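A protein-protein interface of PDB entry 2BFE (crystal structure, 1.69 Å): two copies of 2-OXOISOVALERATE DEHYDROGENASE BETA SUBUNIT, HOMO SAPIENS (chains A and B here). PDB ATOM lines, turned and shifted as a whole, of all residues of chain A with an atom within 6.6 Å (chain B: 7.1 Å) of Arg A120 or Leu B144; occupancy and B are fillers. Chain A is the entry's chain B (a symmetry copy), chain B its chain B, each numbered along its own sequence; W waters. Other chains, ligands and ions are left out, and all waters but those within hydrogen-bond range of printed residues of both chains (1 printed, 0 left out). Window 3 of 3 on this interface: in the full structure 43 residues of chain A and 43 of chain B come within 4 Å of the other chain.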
ATOM      1  N   ASN A 112     -32.714  27.236 -21.846  1.00  0.00           N
ATOM      2  CA  ASN A 112     -31.970  26.047 -21.399  1.00  0.00           C
ATOM      3  C   ASN A 112     -32.353  24.826 -22.228  1.00  0.00           C
ATOM      4  O   ASN A 112     -31.549  23.885 -22.365  1.00  0.00           O
ATOM      5  CB  ASN A 112     -32.189  25.738 -19.908  1.00  0.00           C
ATOM      6  CG  ASN A 112     -31.123  26.325 -19.030  1.00  0.00           C
ATOM      7  OD1 ASN A 112     -30.029  26.697 -19.514  1.00  0.00           O
ATOM      8  ND2 ASN A 112     -31.418  26.438 -17.735  1.00  0.00           N
ATOM      9  N   GLU A 113     -33.564  24.814 -22.792  1.00  0.00           N
ATOM     10  CA  GLU A 113     -33.996  23.598 -23.547  1.00  0.00           C
ATOM     11  C   GLU A 113     -34.003  23.830 -25.050  1.00  0.00           C
ATOM     12  O   GLU A 113     -33.161  23.305 -25.771  1.00  0.00           O
ATOM     13  CB  GLU A 113     -35.383  23.094 -23.048  1.00  0.00           C
ATOM     14  CG  GLU A 113     -35.263  22.664 -21.550  1.00  0.00           C
ATOM     15  CD  GLU A 113     -34.570  21.313 -21.409  1.00  0.00           C
ATOM     16  OE1 GLU A 113     -34.941  20.321 -22.132  1.00  0.00           O
ATOM     17  OE2 GLU A 113     -33.623  21.178 -20.623  1.00  0.00           O
ATOM     18  N   ALA A 114     -34.937  24.643 -25.545  1.00  0.00           N
ATOM     19  CA  ALA A 114     -35.032  24.742 -26.999  1.00  0.00           C
ATOM     20  C   ALA A 114     -33.709  25.114 -27.700  1.00  0.00           C
ATOM     21  O   ALA A 114     -33.334  24.531 -28.719  1.00  0.00           O
ATOM     22  CB  ALA A 114     -36.169  25.796 -27.359  1.00  0.00           C
ATOM     23  N   LYS A 116     -30.668  24.770 -26.854  1.00  0.00           N
ATOM     24  CA  LYS A 116     -29.521  23.903 -26.632  1.00  0.00           C
ATOM     25  C   LYS A 116     -29.807  22.460 -27.073  1.00  0.00           C
ATOM     26  O   LYS A 116     -28.919  21.605 -26.984  1.00  0.00           O
ATOM     27  CB  LYS A 116     -29.109  23.928 -25.148  1.00  0.00           C
ATOM     28  CG  LYS A 116     -28.543  25.303 -24.736  1.00  0.00           C
ATOM     29  CD  LYS A 116     -28.457  25.426 -23.208  1.00  0.00           C
ATOM     30  CE  LYS A 116     -27.784  26.768 -22.802  1.00  0.00           C
ATOM     31  NZ  LYS A 116     -28.425  28.024 -23.401  1.00  0.00           N
ATOM     32  N   TYR A 117     -31.029  22.197 -27.558  1.00  0.00           N
ATOM     33  CA  TYR A 117     -31.501  20.821 -27.847  1.00  0.00           C
ATOM     34  C   TYR A 117     -30.623  20.084 -28.879  1.00  0.00           C
ATOM     35  O   TYR A 117     -30.236  18.916 -28.653  1.00  0.00           O
ATOM     36  CB  TYR A 117     -33.003  20.907 -28.314  1.00  0.00           C
ATOM     37  CG  TYR A 117     -33.889  19.926 -27.619  1.00  0.00           C
ATOM     38  CD1 TYR A 117     -34.606  20.283 -26.470  1.00  0.00           C
ATOM     39  CD2 TYR A 117     -34.004  18.604 -28.124  1.00  0.00           C
ATOM     40  CE1 TYR A 117     -35.390  19.341 -25.827  1.00  0.00           C
ATOM     41  CE2 TYR A 117     -34.819  17.632 -27.527  1.00  0.00           C
ATOM     42  CZ  TYR A 117     -35.526  18.041 -26.351  1.00  0.00           C
ATOM     43  OH  TYR A 117     -36.318  17.118 -25.651  1.00  0.00           O
ATOM     44  N   ARG A 118     -30.291  20.760 -29.978  1.00  0.00           N
ATOM     45  CA  ARG A 118     -29.529  20.095 -31.054  1.00  0.00           C
ATOM     46  C   ARG A 118     -28.089  19.951 -30.599  1.00  0.00           C
ATOM     47  O   ARG A 118     -27.516  18.904 -30.701  1.00  0.00           O
ATOM     48  CB  ARG A 118     -29.610  20.949 -32.320  1.00  0.00           C
ATOM     49  CG  ARG A 118     -29.019  20.192 -33.511  1.00  0.00           C
ATOM     50  CD  ARG A 118     -29.051  21.012 -34.810  1.00  0.00           C
ATOM     51  NE  ARG A 118     -30.398  21.420 -35.275  1.00  0.00           N
ATOM     52  CZ  ARG A 118     -31.205  20.706 -36.063  1.00  0.00           C
ATOM     53  NH1 ARG A 118     -30.888  19.474 -36.485  1.00  0.00           N
ATOM     54  NH2 ARG A 118     -32.387  21.207 -36.444  1.00  0.00           N
ATOM     55  N   TYR A 119     -27.492  21.014 -30.042  1.00  0.00           N
ATOM     56  CA  TYR A 119     -26.090  20.958 -29.669  1.00  0.00           C
ATOM     57  C   TYR A 119     -25.820  19.856 -28.634  1.00  0.00           C
ATOM     58  O   TYR A 119     -24.887  19.051 -28.775  1.00  0.00           O
ATOM     59  CB  TYR A 119     -25.739  22.340 -29.031  1.00  0.00           C
ATOM     60  CG  TYR A 119     -24.282  22.501 -28.705  1.00  0.00           C
ATOM     61  CD1 TYR A 119     -23.367  22.810 -29.730  1.00  0.00           C
ATOM     62  CD2 TYR A 119     -23.814  22.386 -27.374  1.00  0.00           C
ATOM     63  CE1 TYR A 119     -22.000  22.994 -29.447  1.00  0.00           C
ATOM     64  CE2 TYR A 119     -22.466  22.602 -27.075  1.00  0.00           C
ATOM     65  CZ  TYR A 119     -21.574  22.922 -28.110  1.00  0.00           C
ATOM     66  OH  TYR A 119     -20.228  23.152 -27.849  1.00  0.00           O
ATOM     67  N   ARG A 120     -26.636  19.832 -27.573  1.00  0.00           N
ATOM     68  CA  ARG A 120     -26.308  18.992 -26.462  1.00  0.00           C
ATOM     69  C   ARG A 120     -26.562  17.519 -26.788  1.00  0.00           C
ATOM     70  O   ARG A 120     -26.034  16.628 -26.085  1.00  0.00           O
ATOM     71  CB  ARG A 120     -27.121  19.411 -25.216  1.00  0.00           C
ATOM     72  CG  ARG A 120     -28.580  18.830 -25.264  1.00  0.00           C
ATOM     73  CD  ARG A 120     -29.434  19.587 -24.266  1.00  0.00           C
ATOM     74  NE  ARG A 120     -30.804  19.042 -24.290  1.00  0.00           N
ATOM     75  CZ  ARG A 120     -31.794  19.529 -23.525  1.00  0.00           C
ATOM     76  NH1 ARG A 120     -31.547  20.593 -22.704  1.00  0.00           N
ATOM     77  NH2 ARG A 120     -32.983  18.915 -23.574  1.00  0.00           N
ATOM     78  N   SER A 121     -27.280  17.219 -27.868  1.00  0.00           N
ATOM     79  CA  SER A 121     -27.496  15.804 -28.215  1.00  0.00           C
ATOM     80  C   SER A 121     -26.571  15.368 -29.359  1.00  0.00           C
ATOM     81  O   SER A 121     -26.697  14.263 -29.859  1.00  0.00           O
ATOM     82  CB  SER A 121     -28.954  15.654 -28.655  1.00  0.00           C
ATOM     83  OG  SER A 121     -29.265  16.307 -29.889  1.00  0.00           O
ATOM     84  N   GLY A 122     -25.682  16.249 -29.806  1.00  0.00           N
ATOM     85  CA  GLY A 122     -24.865  15.916 -30.950  1.00  0.00           C
ATOM     86  C   GLY A 122     -25.689  15.780 -32.216  1.00  0.00           C
ATOM     87  O   GLY A 122     -25.318  15.022 -33.140  1.00  0.00           O
ATOM     88  N   ASP A 123     -26.809  16.476 -32.269  1.00  0.00           N
ATOM     89  CA  ASP A 123     -27.749  16.368 -33.354  1.00  0.00           C
ATOM     90  C   ASP A 123     -28.476  15.012 -33.402  1.00  0.00           C
ATOM     91  O   ASP A 123     -29.060  14.681 -34.441  1.00  0.00           O
ATOM     92  CB  ASP A 123     -27.045  16.630 -34.727  1.00  0.00           C
ATOM     93  CG  ASP A 123     -28.040  16.929 -35.852  1.00  0.00           C
ATOM     94  OD1 ASP A 123     -29.037  17.577 -35.590  1.00  0.00           O
ATOM     95  OD2 ASP A 123     -27.894  16.491 -37.063  1.00  0.00           O
ATOM     96  N   ASP B 101     -27.273  28.588 -13.564  1.00  0.00           N
ATOM     97  CA  ASP B 101     -27.873  27.966 -14.725  1.00  0.00           C
ATOM     98  C   ASP B 101     -29.323  27.662 -14.492  1.00  0.00           C
ATOM     99  O   ASP B 101     -30.077  27.473 -15.466  1.00  0.00           O
ATOM    100  CB  ASP B 101     -27.217  26.604 -14.921  1.00  0.00           C
ATOM    101  CG  ASP B 101     -25.675  26.728 -14.913  1.00  0.00           C
ATOM    102  OD1 ASP B 101     -25.064  26.992 -13.852  1.00  0.00           O
ATOM    103  OD2 ASP B 101     -25.000  26.609 -15.982  1.00  0.00           O
ATOM    104  N   HIS B 141     -15.311  21.608 -15.758  1.00  0.00           N
ATOM    105  CA  HIS B 141     -15.974  20.413 -16.295  1.00  0.00           C
ATOM    106  C   HIS B 141     -17.493  20.498 -16.146  1.00  0.00           C
ATOM    107  O   HIS B 141     -18.194  19.488 -16.347  1.00  0.00           O
ATOM    108  CB  HIS B 141     -15.504  19.176 -15.509  1.00  0.00           C
ATOM    109  CG  HIS B 141     -15.439  19.425 -14.042  1.00  0.00           C
ATOM    110  ND1 HIS B 141     -14.259  19.693 -13.376  1.00  0.00           N
ATOM    111  CD2 HIS B 141     -16.426  19.564 -13.132  1.00  0.00           C
ATOM    112  CE1 HIS B 141     -14.531  19.948 -12.108  1.00  0.00           C
ATOM    113  NE2 HIS B 141     -15.838  19.868 -11.937  1.00  0.00           N
ATOM    114  N   GLY B 142     -18.006  21.692 -15.822  1.00  0.00           N
ATOM    115  CA  GLY B 142     -19.457  21.873 -15.540  1.00  0.00           C
ATOM    116  C   GLY B 142     -20.362  21.722 -16.757  1.00  0.00           C
ATOM    117  O   GLY B 142     -21.580  21.594 -16.583  1.00  0.00           O
ATOM    118  N   ALA B 143     -19.798  21.873 -17.950  1.00  0.00           N
ATOM    119  CA  ALA B 143     -20.571  21.743 -19.179  1.00  0.00           C
ATOM    120  C   ALA B 143     -21.769  22.719 -19.236  1.00  0.00           C
ATOM    121  O   ALA B 143     -21.687  23.855 -18.749  1.00  0.00           O
ATOM    122  CB  ALA B 143     -21.011  20.225 -19.400  1.00  0.00           C
ATOM    123  N   LEU B 144     -22.893  22.316 -19.812  1.00  0.00           N
ATOM    124  CA  LEU B 144     -23.906  23.337 -20.204  1.00  0.00           C
ATOM    125  C   LEU B 144     -24.652  23.960 -19.046  1.00  0.00           C
ATOM    126  O   LEU B 144     -25.102  25.124 -19.168  1.00  0.00           O
ATOM    127  CB  LEU B 144     -24.950  22.751 -21.155  1.00  0.00           C
ATOM    128  CG  LEU B 144     -24.513  22.620 -22.640  1.00  0.00           C
ATOM    129  CD1 LEU B 144     -23.578  21.404 -22.847  1.00  0.00           C
ATOM    130  CD2 LEU B 144     -25.839  22.396 -23.361  1.00  0.00           C
ATOM    131  N   TYR B 145     -24.827  23.233 -17.937  1.00  0.00           N
ATOM    132  CA  TYR B 145     -25.746  23.628 -16.878  1.00  0.00           C
ATOM    133  C   TYR B 145     -25.101  23.750 -15.522  1.00  0.00           C
ATOM    134  O   TYR B 145     -25.807  23.924 -14.493  1.00  0.00           O
ATOM    135  CB  TYR B 145     -26.994  22.707 -16.834  1.00  0.00           C
ATOM    136  CG  TYR B 145     -27.701  22.566 -18.195  1.00  0.00           C
ATOM    137  CD1 TYR B 145     -28.402  23.664 -18.737  1.00  0.00           C
ATOM    138  CD2 TYR B 145     -27.549  21.423 -18.944  1.00  0.00           C
ATOM    139  CE1 TYR B 145     -28.973  23.586 -20.012  1.00  0.00           C
ATOM    140  CE2 TYR B 145     -28.154  21.309 -20.204  1.00  0.00           C
ATOM    141  CZ  TYR B 145     -28.875  22.406 -20.699  1.00  0.00           C
ATOM    142  OH  TYR B 145     -29.428  22.341 -21.976  1.00  0.00           O
ATOM    143  N   HIS B 146     -23.760  23.671 -15.456  1.00  0.00           N
ATOM    144  CA  HIS B 146     -23.083  23.964 -14.192  1.00  0.00           C
ATOM    145  C   HIS B 146     -22.085  25.117 -14.374  1.00  0.00           C
ATOM    146  O   HIS B 146     -21.286  25.369 -13.472  1.00  0.00           O
ATOM    147  CB  HIS B 146     -22.320  22.733 -13.641  1.00  0.00           C
ATOM    148  CG  HIS B 146     -23.157  21.822 -12.783  1.00  0.00           C
ATOM    149  ND1 HIS B 146     -22.603  20.853 -11.977  1.00  0.00           N
ATOM    150  CD2 HIS B 146     -24.498  21.726 -12.615  1.00  0.00           C
ATOM    151  CE1 HIS B 146     -23.569  20.193 -11.349  1.00  0.00           C
ATOM    152  NE2 HIS B 146     -24.727  20.741 -11.681  1.00  0.00           N
ATOM    153  N   SER B 147     -22.117  25.791 -15.527  1.00  0.00           N
ATOM    154  CA  SER B 147     -21.030  26.738 -15.917  1.00  0.00           C
ATOM    155  C   SER B 147     -21.494  28.143 -16.246  1.00  0.00           C
ATOM    156  O   SER B 147     -20.637  29.023 -16.507  1.00  0.00           O
ATOM    157  CB  SER B 147     -20.352  26.247 -17.192  1.00  0.00           C
ATOM    158  OG  SER B 147     -19.914  24.905 -17.031  1.00  0.00           O
ATOM    159  N   GLN B 148     -22.808  28.338 -16.377  1.00  0.00           N
ATOM    160  CA  GLN B 148     -23.291  29.567 -17.041  1.00  0.00           C
ATOM    161  C   GLN B 148     -22.998  30.893 -16.285  1.00  0.00           C
ATOM    162  O   GLN B 148     -22.861  30.913 -15.047  1.00  0.00           O
ATOM    163  CB  GLN B 148     -24.783  29.504 -17.363  1.00  0.00           C
ATOM    164  CG  GLN B 148     -25.067  28.468 -18.498  1.00  0.00           C
ATOM    165  CD  GLN B 148     -26.539  28.480 -18.857  1.00  0.00           C
ATOM    166  OE1 GLN B 148     -27.111  29.546 -19.152  1.00  0.00           O
ATOM    167  NE2 GLN B 148     -27.158  27.262 -18.896  1.00  0.00           N
ATOM    168  N   PRO B 316     -23.458  27.019 -26.589  1.00  0.00           N
ATOM    169  CA  PRO B 316     -23.659  26.543 -25.199  1.00  0.00           C
ATOM    170  C   PRO B 316     -22.294  26.164 -24.593  1.00  0.00           C
ATOM    171  O   PRO B 316     -21.300  26.021 -25.324  1.00  0.00           O
ATOM    172  CB  PRO B 316     -24.582  25.322 -25.370  1.00  0.00           C
ATOM    173  CG  PRO B 316     -25.249  25.578 -26.731  1.00  0.00           C
ATOM    174  CD  PRO B 316     -24.071  26.098 -27.600  1.00  0.00           C
ATOM    175  N   PHE B 317     -22.222  26.030 -23.260  1.00  0.00           N
ATOM    176  CA  PHE B 317     -20.904  25.822 -22.636  1.00  0.00           C
ATOM    177  C   PHE B 317     -20.508  24.361 -22.623  1.00  0.00           C
ATOM    178  O   PHE B 317     -21.214  23.570 -22.035  1.00  0.00           O
ATOM    179  CB  PHE B 317     -20.992  26.402 -21.183  1.00  0.00           C
ATOM    180  CG  PHE B 317     -19.633  26.675 -20.597  1.00  0.00           C
ATOM    181  CD1 PHE B 317     -18.817  25.585 -20.303  1.00  0.00           C
ATOM    182  CD2 PHE B 317     -19.141  27.984 -20.468  1.00  0.00           C
ATOM    183  CE1 PHE B 317     -17.545  25.748 -19.844  1.00  0.00           C
ATOM    184  CE2 PHE B 317     -17.848  28.201 -19.971  1.00  0.00           C
ATOM    185  CZ  PHE B 317     -17.035  27.093 -19.646  1.00  0.00           C
ATOM    186  N   PRO B 318     -19.431  23.969 -23.302  1.00  0.00           N
ATOM    187  CA  PRO B 318     -19.171  22.523 -23.522  1.00  0.00           C
ATOM    188  C   PRO B 318     -18.470  21.832 -22.380  1.00  0.00           C
ATOM    189  O   PRO B 318     -17.703  22.432 -21.669  1.00  0.00           O
ATOM    190  CB  PRO B 318     -18.258  22.508 -24.781  1.00  0.00           C
ATOM    191  CG  PRO B 318     -17.462  23.786 -24.610  1.00  0.00           C
ATOM    192  CD  PRO B 318     -18.476  24.840 -24.004  1.00  0.00           C
ATOM    193  N   HIS B 319     -18.717  20.522 -22.233  1.00  0.00           N
ATOM    194  CA  HIS B 319     -17.949  19.672 -21.324  1.00  0.00           C
ATOM    195  C   HIS B 319     -16.465  19.501 -21.751  1.00  0.00           C
ATOM    196  O   HIS B 319     -15.576  20.153 -21.197  1.00  0.00           O
ATOM    197  CB  HIS B 319     -18.671  18.283 -21.184  1.00  0.00           C
ATOM    198  CG  HIS B 319     -17.901  17.318 -20.339  1.00  0.00           C
ATOM    199  ND1 HIS B 319     -17.674  16.004 -20.679  1.00  0.00           N
ATOM    200  CD2 HIS B 319     -17.287  17.517 -19.144  1.00  0.00           C
ATOM    201  CE1 HIS B 319     -16.947  15.430 -19.726  1.00  0.00           C
ATOM    202  NE2 HIS B 319     -16.694  16.344 -18.792  1.00  0.00           N
HETATM  203  O   HOH W   1     -27.361  30.094 -21.849  1.00  0.00           O
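Hydrophobic or aromatic side chains of chain A that line the printed part of chain B: Tyr A119.
Hydrophobic or aromatic side chains of chain B within 4 Å of the printed part of chain A: Leu B144, Tyr B145, Pro B316 and Pro B318.
Along chain B the printed residues that touch a printed residue of chain A span positions 101 to 318.
NH1 of Arg A120 sits at hydrogen-bond distance from OH of Tyr B145, 2.8 Å away.
The side-chain amide nitrogen (NE2) of Gln B148 is in hydrogen-bond range of the side-chain amide oxygen (OD1) of Asn A112 (3.0 Å).
The side-chain amide nitrogen (ND2) of Asn A112 sits at hydrogen-bond distance from the backbone carbonyl oxygen (O) of Asp B101 (2.8 Å).
The backbone carbonyl oxygen (O) of Asn A112 lies within hydrogen-bond range of the side-chain hydroxyl (OH) of Tyr B145.
The side-chain carboxylate (OE1) of Glu A113 is in salt-bridge range of the guanidinium group (NH2) of Arg A120 (2.8 Å).
The side-chain carboxylate (OD2) of Asp B101 sits at hydrogen-bond distance from the backbone NH (N) of Ser B147 (3.0 Å).
The backbone NH (N) of Leu B144 sits at hydrogen-bond distance from the backbone carbonyl oxygen (O) of Phe B317, 3.1 Å away.
OD2 of Asp B101 sits at hydrogen-bond distance from N of Gln B148.
The backbone carbonyl oxygen (O) of Leu B144 lies within hydrogen-bond range of the side-chain amide nitrogen (NE2) of Gln B148 (3.0 Å).
The backbone carbonyl oxygen (O) of Asn A112 lies within hydrogen-bond range of the guanidinium group (NH1) of Arg A120 (3.3 Å).
Lys A116 touches Tyr B145.
CE of Lys A116 touches NE2 of Gln B148, at 3.99 Å.
CG of Lys A116 touches CG of Pro B316, at 3.9 Å.
Pro B316 touches Tyr A119.
OH of Tyr A119 touches CB of Pro B318 (3.7 Å).
Leu B144 touches Arg A120.
Printed residues of chain B within 4 Å of Asn A112: Asp B101 (2.8 Å), Tyr B145 (2.7 Å) and Gln B148 (3.0 Å).
Printed residues of chain B within 4 Å of Lys A116: Tyr B145, Gln B148 and Pro B316.
Arg A120 touches just these residues of chain B: Leu B144 (3.7 Å) and Tyr B145 (2.8 Å).
Printed residues of chain A within 4 Å of Leu B144: Arg A120.
Printed residues of chain A within 4 Å of Tyr B145: Asn A112 (2.7 Å), Lys A116 (3.5 Å) and Arg A120 (2.8 Å).
Printed residues of chain A within 4 Å of Pro B316: Lys A116 (3.9 Å) and Tyr A119 (3.6 Å).
Of the printed residues of chain A, Pro B318 touches Tyr A119.
The nearest residue of chain B that does not touch Arg A120 is Pro B316 (6.0 Å).
The nearest printed residue of chain A that does not touch Leu B144 is Lys A116 (4.01 Å).
The nearest printed residue of chain A that does not touch Pro B316 is Arg A120 (6.0 Å).
Water W1 bridges OE1 of Gln B148 (2.8 Å) and NZ of Lys A116 (2.8 Å).
No position is printed for both chains.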
